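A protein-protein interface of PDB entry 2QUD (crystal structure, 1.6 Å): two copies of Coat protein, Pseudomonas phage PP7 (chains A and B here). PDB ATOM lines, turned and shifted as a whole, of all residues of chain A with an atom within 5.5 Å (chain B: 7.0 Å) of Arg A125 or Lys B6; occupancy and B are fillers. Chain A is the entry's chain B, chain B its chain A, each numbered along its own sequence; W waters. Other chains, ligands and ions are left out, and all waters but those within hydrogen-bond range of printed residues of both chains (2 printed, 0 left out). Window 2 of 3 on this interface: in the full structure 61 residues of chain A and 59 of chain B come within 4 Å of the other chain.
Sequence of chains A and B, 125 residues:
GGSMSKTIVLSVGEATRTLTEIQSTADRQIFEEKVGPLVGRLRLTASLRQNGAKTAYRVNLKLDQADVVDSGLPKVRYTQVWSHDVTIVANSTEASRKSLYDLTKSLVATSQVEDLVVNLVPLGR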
ATOM      1  N   SER A 111       3.116  12.353 -21.802  1.00  0.00           N
ATOM      2  CA  SER A 111       1.993  12.872 -21.040  1.00  0.00           C
ATOM      3  C   SER A 111       2.459  13.482 -19.715  1.00  0.00           C
ATOM      4  O   SER A 111       1.866  14.452 -19.228  1.00  0.00           O
ATOM      5  CB  SER A 111       0.940  11.790 -20.775  1.00  0.00           C
ATOM      6  OG  SER A 111       1.439  10.753 -19.960  1.00  0.00           O
ATOM      7  N   GLN A 112       3.525  12.929 -19.134  1.00  0.00           N
ATOM      8  CA  GLN A 112       4.051  13.480 -17.883  1.00  0.00           C
ATOM      9  C   GLN A 112       4.527  14.926 -18.037  1.00  0.00           C
ATOM     10  O   GLN A 112       4.261  15.809 -17.191  1.00  0.00           O
ATOM     11  CB  GLN A 112       5.175  12.605 -17.340  1.00  0.00           C
ATOM     12  CG  GLN A 112       4.706  11.310 -16.721  1.00  0.00           C
ATOM     13  CD  GLN A 112       5.785  10.579 -15.967  1.00  0.00           C
ATOM     14  OE1 GLN A 112       6.678  11.212 -15.383  1.00  0.00           O
ATOM     15  NE2 GLN A 112       5.718   9.252 -15.963  1.00  0.00           N
ATOM     16  N   ASP A 115       1.527  17.150 -18.279  1.00  0.00           N
ATOM     17  CA  ASP A 115       0.924  17.379 -16.957  1.00  0.00           C
ATOM     18  C   ASP A 115       1.764  18.298 -16.072  1.00  0.00           C
ATOM     19  O   ASP A 115       1.211  19.021 -15.259  1.00  0.00           O
ATOM     20  CB  ASP A 115       0.655  16.064 -16.245  1.00  0.00           C
ATOM     21  CG  ASP A 115      -0.431  15.246 -16.916  1.00  0.00           C
ATOM     22  OD1 ASP A 115      -1.298  15.827 -17.592  1.00  0.00           O
ATOM     23  OD2 ASP A 115      -0.424  14.013 -16.750  1.00  0.00           O
ATOM     24  N   VAL A 121       2.056  19.145 -12.192  1.00  0.00           N
ATOM     25  CA  VAL A 121       2.263  17.848 -11.550  1.00  0.00           C
ATOM     26  C   VAL A 121       3.713  17.406 -11.793  1.00  0.00           C
ATOM     27  O   VAL A 121       4.124  17.257 -12.971  1.00  0.00           O
ATOM     28  CB  VAL A 121       1.331  16.794 -12.125  1.00  0.00           C
ATOM     29  CG1 VAL A 121       1.584  15.476 -11.441  1.00  0.00           C
ATOM     30  CG2 VAL A 121      -0.133  17.225 -11.959  1.00  0.00           C
ATOM     31  N   PRO A 122       4.510  17.203 -10.739  1.00  0.00           N
ATOM     32  CA  PRO A 122       5.882  16.751 -10.968  1.00  0.00           C
ATOM     33  C   PRO A 122       5.997  15.449 -11.737  1.00  0.00           C
ATOM     34  O   PRO A 122       5.109  14.635 -11.652  1.00  0.00           O
ATOM     35  CB  PRO A 122       6.426  16.575  -9.552  1.00  0.00           C
ATOM     36  CG  PRO A 122       5.654  17.602  -8.746  1.00  0.00           C
ATOM     37  CD  PRO A 122       4.277  17.529  -9.305  1.00  0.00           C
ATOM     38  N   LEU A 123       7.086  15.282 -12.459  1.00  0.00           N
ATOM     39  CA  LEU A 123       7.352  14.030 -13.158  1.00  0.00           C
ATOM     40  C   LEU A 123       7.447  12.841 -12.216  1.00  0.00           C
ATOM     41  O   LEU A 123       7.715  12.970 -11.006  1.00  0.00           O
ATOM     42  CB  LEU A 123       8.663  14.124 -13.945  1.00  0.00           C
ATOM     43  CG  LEU A 123       8.738  15.228 -15.002  1.00  0.00           C
ATOM     44  CD1 LEU A 123      10.117  15.123 -15.687  1.00  0.00           C
ATOM     45  CD2 LEU A 123       7.552  15.225 -15.985  1.00  0.00           C
ATOM     46  N   GLY A 124       7.191  11.673 -12.793  1.00  0.00           N
ATOM     47  CA  GLY A 124       7.400  10.397 -12.113  1.00  0.00           C
ATOM     48  C   GLY A 124       6.065   9.782 -11.751  1.00  0.00           C
ATOM     49  O   GLY A 124       5.260  10.415 -11.080  1.00  0.00           O
ATOM     50  N   ARG A 125       5.857   8.538 -12.176  1.00  0.00           N
ATOM     51  CA  ARG A 125       4.607   7.776 -11.868  1.00  0.00           C
ATOM     52  C   ARG A 125       4.965   6.353 -11.472  1.00  0.00           C
ATOM     53  O   ARG A 125       4.115   5.709 -10.839  1.00  0.00           O
ATOM     54  CB  ARG A 125       3.674   7.741 -13.077  1.00  0.00           C
ATOM     55  CG  ARG A 125       3.237   9.068 -13.603  1.00  0.00           C
ATOM     56  CD  ARG A 125       2.281   9.809 -12.671  1.00  0.00           C
ATOM     57  NE  ARG A 125       1.810  11.033 -13.312  1.00  0.00           N
ATOM     58  CZ  ARG A 125       2.508  12.172 -13.402  1.00  0.00           C
ATOM     59  NH1 ARG A 125       2.001  13.209 -14.053  1.00  0.00           N
ATOM     60  NH2 ARG A 125       3.693  12.270 -12.838  1.00  0.00           N
ATOM     61  OXT ARG A 125       6.041   5.810 -11.751  1.00  0.00           O
ATOM     62  N   SER B   3       4.954   2.428  -2.381  1.00  0.00           N
ATOM     63  CA  SER B   3       5.140   2.606  -3.813  1.00  0.00           C
ATOM     64  C   SER B   3       6.538   2.255  -4.289  1.00  0.00           C
ATOM     65  O   SER B   3       7.530   2.485  -3.592  1.00  0.00           O
ATOM     66  CB  SER B   3       4.815   4.047  -4.195  1.00  0.00           C
ATOM     67  OG  SER B   3       3.503   4.366  -3.782  1.00  0.00           O
ATOM     68  N   MET B   4       6.582   1.635  -5.461  1.00  0.00           N
ATOM     69  CA  MET B   4       7.812   1.412  -6.185  1.00  0.00           C
ATOM     70  C   MET B   4       8.420   2.754  -6.546  1.00  0.00           C
ATOM     71  O   MET B   4       7.777   3.807  -6.420  1.00  0.00           O
ATOM     72  CB  MET B   4       7.544   0.590  -7.465  1.00  0.00           C
ATOM     73  CG  MET B   4       6.574   1.234  -8.486  1.00  0.00           C
ATOM     74  SD  MET B   4       5.714  -0.009  -9.480  1.00  0.00           S
ATOM     75  CE  MET B   4       4.088   0.722  -9.686  1.00  0.00           C
ATOM     76  N   SER B   5       9.667   2.722  -6.984  1.00  0.00           N
ATOM     77  CA  SER B   5      10.326   3.940  -7.437  1.00  0.00           C
ATOM     78  C   SER B   5       9.600   4.471  -8.673  1.00  0.00           C
ATOM     79  O   SER B   5       9.242   3.710  -9.570  1.00  0.00           O
ATOM     80  CB  SER B   5      11.802   3.696  -7.750  1.00  0.00           C
ATOM     81  OG  SER B   5      12.554   3.473  -6.566  1.00  0.00           O
ATOM     82  N   LYS B   6       9.410   5.780  -8.692  1.00  0.00           N
ATOM     83  CA  LYS B   6       8.740   6.490  -9.773  1.00  0.00           C
ATOM     84  C   LYS B   6       9.572   6.406 -11.051  1.00  0.00           C
ATOM     85  O   LYS B   6      10.772   6.412 -10.994  1.00  0.00           O
ATOM     86  CB  LYS B   6       8.554   7.961  -9.370  1.00  0.00           C
ATOM     87  CG  LYS B   6       7.591   8.174  -8.209  1.00  0.00           C
ATOM     88  CD  LYS B   6       7.311   9.633  -8.079  1.00  0.00           C
ATOM     89  CE  LYS B   6       6.198   9.987  -7.046  1.00  0.00           C
ATOM     90  NZ  LYS B   6       6.253   9.392  -5.678  1.00  0.00           N
ATOM     91  N   THR B   7       8.912   6.306 -12.196  1.00  0.00           N
ATOM     92  CA  THR B   7       9.602   6.295 -13.475  1.00  0.00           C
ATOM     93  C   THR B   7       8.954   7.265 -14.489  1.00  0.00           C
ATOM     94  O   THR B   7       7.814   7.675 -14.368  1.00  0.00           O
ATOM     95  CB  THR B   7       9.590   4.874 -14.119  1.00  0.00           C
ATOM     96  OG1 THR B   7       8.229   4.494 -14.394  1.00  0.00           O
ATOM     97  CG2 THR B   7      10.280   3.802 -13.236  1.00  0.00           C
ATOM     98  N   ILE B   8       9.730   7.556 -15.522  1.00  0.00           N
ATOM     99  CA  ILE B   8       9.256   8.174 -16.756  1.00  0.00           C
ATOM    100  C   ILE B   8       9.839   7.362 -17.930  1.00  0.00           C
ATOM    101  O   ILE B   8      10.998   6.976 -17.901  1.00  0.00           O
ATOM    102  CB  ILE B   8       9.568   9.680 -16.825  1.00  0.00           C
ATOM    103  CG1 ILE B   8       8.959  10.311 -18.078  1.00  0.00           C
ATOM    104  CG2 ILE B   8      11.028   9.966 -16.709  1.00  0.00           C
ATOM    105  CD1 ILE B   8       8.925  11.849 -18.047  1.00  0.00           C
ATOM    106  N   THR B  18      13.752   3.755 -19.903  1.00  0.00           N
ATOM    107  CA  THR B  18      13.070   4.021 -18.636  1.00  0.00           C
ATOM    108  C   THR B  18      14.024   4.764 -17.711  1.00  0.00           C
ATOM    109  O   THR B  18      15.102   4.275 -17.455  1.00  0.00           O
ATOM    110  CB  THR B  18      12.606   2.714 -17.969  1.00  0.00           C
ATOM    111  OG1 THR B  18      11.715   2.031 -18.857  1.00  0.00           O
ATOM    112  CG2 THR B  18      11.946   2.980 -16.607  1.00  0.00           C
ATOM    113  N   LEU B  19      13.582   5.907 -17.197  1.00  0.00           N
ATOM    114  CA  LEU B  19      14.344   6.682 -16.233  1.00  0.00           C
ATOM    115  C   LEU B  19      13.652   6.614 -14.889  1.00  0.00           C
ATOM    116  O   LEU B  19      12.480   6.969 -14.763  1.00  0.00           O
ATOM    117  CB  LEU B  19      14.490   8.126 -16.670  1.00  0.00           C
ATOM    118  CG  LEU B  19      15.457   8.333 -17.835  1.00  0.00           C
ATOM    119  CD1 LEU B  19      14.689   8.462 -19.143  1.00  0.00           C
ATOM    120  CD2 LEU B  19      16.286   9.551 -17.542  1.00  0.00           C
ATOM    121  N   THR B  20      14.414   6.196 -13.883  1.00  0.00           N
ATOM    122  CA  THR B  20      13.924   5.917 -12.525  1.00  0.00           C
ATOM    123  C   THR B  20      14.349   6.988 -11.559  1.00  0.00           C
ATOM    124  O   THR B  20      15.506   7.400 -11.565  1.00  0.00           O
ATOM    125  CB  THR B  20      14.482   4.548 -12.042  1.00  0.00           C
ATOM    126  OG1 THR B  20      14.067   3.533 -12.976  1.00  0.00           O
ATOM    127  CG2 THR B  20      13.978   4.209 -10.697  1.00  0.00           C
ATOM    128  N   GLU B  21      13.403   7.409 -10.743  1.00  0.00           N
ATOM    129  CA  GLU B  21      13.691   8.440  -9.739  1.00  0.00           C
ATOM    130  C   GLU B  21      14.696   7.900  -8.717  1.00  0.00           C
ATOM    131  O   GLU B  21      14.485   6.824  -8.129  1.00  0.00           O
ATOM    132  CB  GLU B  21      12.431   8.898  -9.038  1.00  0.00           C
ATOM    133  CG  GLU B  21      12.553  10.230  -8.303  1.00  0.00           C
ATOM    134  CD  GLU B  21      11.262  10.611  -7.609  1.00  0.00           C
ATOM    135  OE1 GLU B  21      10.694  11.703  -7.898  1.00  0.00           O
ATOM    136  OE2 GLU B  21      10.846   9.843  -6.724  1.00  0.00           O
ATOM    137  N   ILE B  22      15.800   8.638  -8.549  1.00  0.00           N
ATOM    138  CA  ILE B  22      16.821   8.326  -7.551  1.00  0.00           C
ATOM    139  C   ILE B  22      16.947   9.368  -6.417  1.00  0.00           C
ATOM    140  O   ILE B  22      17.586   9.093  -5.388  1.00  0.00           O
ATOM    141  CB  ILE B  22      18.197   8.055  -8.223  1.00  0.00           C
ATOM    142  CG1 ILE B  22      18.731   9.255  -8.973  1.00  0.00           C
ATOM    143  CG2 ILE B  22      18.042   6.875  -9.234  1.00  0.00           C
ATOM    144  CD1 ILE B  22      20.214   9.164  -9.280  1.00  0.00           C
ATOM    145  N   SER B  24      14.452  12.818  -4.659  1.00  0.00           N
ATOM    146  CA  SER B  24      13.320  13.721  -4.640  1.00  0.00           C
ATOM    147  C   SER B  24      13.479  14.558  -3.373  1.00  0.00           C
ATOM    148  O   SER B  24      13.257  14.066  -2.272  1.00  0.00           O
ATOM    149  CB  SER B  24      12.003  12.962  -4.639  1.00  0.00           C
ATOM    150  OG  SER B  24      10.921  13.868  -4.605  1.00  0.00           O
ATOM    151  N   GLN B  29      14.154  16.867  -8.372  1.00  0.00           N
ATOM    152  CA  GLN B  29      14.134  15.444  -8.600  1.00  0.00           C
ATOM    153  C   GLN B  29      15.254  15.086  -9.550  1.00  0.00           C
ATOM    154  O   GLN B  29      15.601  15.872 -10.410  1.00  0.00           O
ATOM    155  CB  GLN B  29      12.822  14.995  -9.234  1.00  0.00           C
ATOM    156  CG  GLN B  29      11.624  15.252  -8.408  1.00  0.00           C
ATOM    157  CD  GLN B  29      10.369  15.196  -9.230  1.00  0.00           C
ATOM    158  OE1 GLN B  29       9.946  16.216  -9.781  1.00  0.00           O
ATOM    159  NE2 GLN B  29       9.818  13.996  -9.391  1.00  0.00           N
ATOM    160  N   PHE B  31      16.275  11.686 -12.017  1.00  0.00           N
ATOM    161  CA  PHE B  31      15.908  10.402 -12.587  1.00  0.00           C
ATOM    162  C   PHE B  31      17.146   9.876 -13.322  1.00  0.00           C
ATOM    163  O   PHE B  31      17.882  10.669 -13.949  1.00  0.00           O
ATOM    164  CB  PHE B  31      14.762  10.482 -13.606  1.00  0.00           C
ATOM    165  CG  PHE B  31      13.413  10.904 -13.023  1.00  0.00           C
ATOM    166  CD1 PHE B  31      13.208  12.253 -12.657  1.00  0.00           C
ATOM    167  CD2 PHE B  31      12.384   9.994 -12.833  1.00  0.00           C
ATOM    168  CE1 PHE B  31      11.988  12.642 -12.122  1.00  0.00           C
ATOM    169  CE2 PHE B  31      11.181  10.385 -12.296  1.00  0.00           C
ATOM    170  CZ  PHE B  31      10.972  11.693 -11.973  1.00  0.00           C
HETATM  171  O   HOH W   1       6.823   3.417 -11.386  1.00  0.00           O
HETATM  172  O   HOH W   2       9.082  17.141 -12.195  1.00  0.00           O
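The side-chain amide nitrogen of Gln B29 is in hydrogen-bond range of the backbone carbonyl oxygen of Leu A123 (2.8 Å). The side-chain amide nitrogen (NE2) of Gln A112 sits at hydrogen-bond distance from the backbone carbonyl oxygen (O) of Thr B7, 3.1 Å away. N of Thr B7 sits at hydrogen-bond distance from OXT of Arg A125 (2.9 Å).
The backbone NH (N) of Gly A124 is in hydrogen-bond range of the side-chain amide oxygen (OE1) of Gln A112 (2.7 Å). The backbone carbonyl oxygen of Lys B6 sits at hydrogen-bond distance from the backbone NH of Glu B21 (2.8 Å). NH2 of Arg A125 is in hydrogen-bond range of O of Pro A122 (3.0 Å). The backbone NH (N) of Leu B19 sits at hydrogen-bond distance from the backbone carbonyl oxygen (O) of Ile B8 (2.9 Å). The side-chain carboxylate of Glu B21 is in hydrogen-bond range of the side-chain amide nitrogen of Gln B29 (2.9 Å). OD2 of Asp A115 is in salt-bridge range of NH1 of Arg A125 (3.7 Å).
Among the printed residues, merely in contact across the chains: Arg A125 with Lys B6, Gln A112 with Ile B8, Pro A122 with Gln B29, Gly A124 with Thr B7, Leu A123 with Phe B31, Gly A124 with Lys B6 and Gly A124 with Phe B31.
Of the printed residues of chain B, Leu A123 touches Gln B29 and Phe B31. Printed residues of chain B within 4 Å of Arg A125: Lys B6 (3.4 Å) and Thr B7 (2.9 Å). Of the printed residues of chain A, Thr B7 touches Gln A112 (3.1 Å), Gly A124 (3.6 Å) and Arg A125 (2.9 Å). Thr B18 touches none of the printed residues of chain A. The nearest printed residue of chain B that does not touch Arg A125 is Ser B5 (4.4 Å).
Of the 14 printed residues of chain B, 5 touch a printed residue of chain A. Of the 8 printed residues of chain A, 5 touch a printed residue of chain B. Hydrophobic or aromatic side chains of chain A within 4 Å of the printed part of chain B: Pro A122 and Leu A123.
No position is printed for both chains. Of the 10 pairs that touch across the chains among the printed residues, none has its exchanged pair printed and touching as well.
Water W1 lies within hydrogen-bond range of the chain-end carboxylate of Arg A125 (2.5 Å), the backbone carbonyl oxygen of Ser B5 (3.0 Å) and the side-chain hydroxyl of Thr B7 (3.5 Å). Water W2 bridges the side-chain amide oxygen (OE1) of Gln B29 (2.7 Å) and the backbone NH (N) of Leu A123 (2.7 Å).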
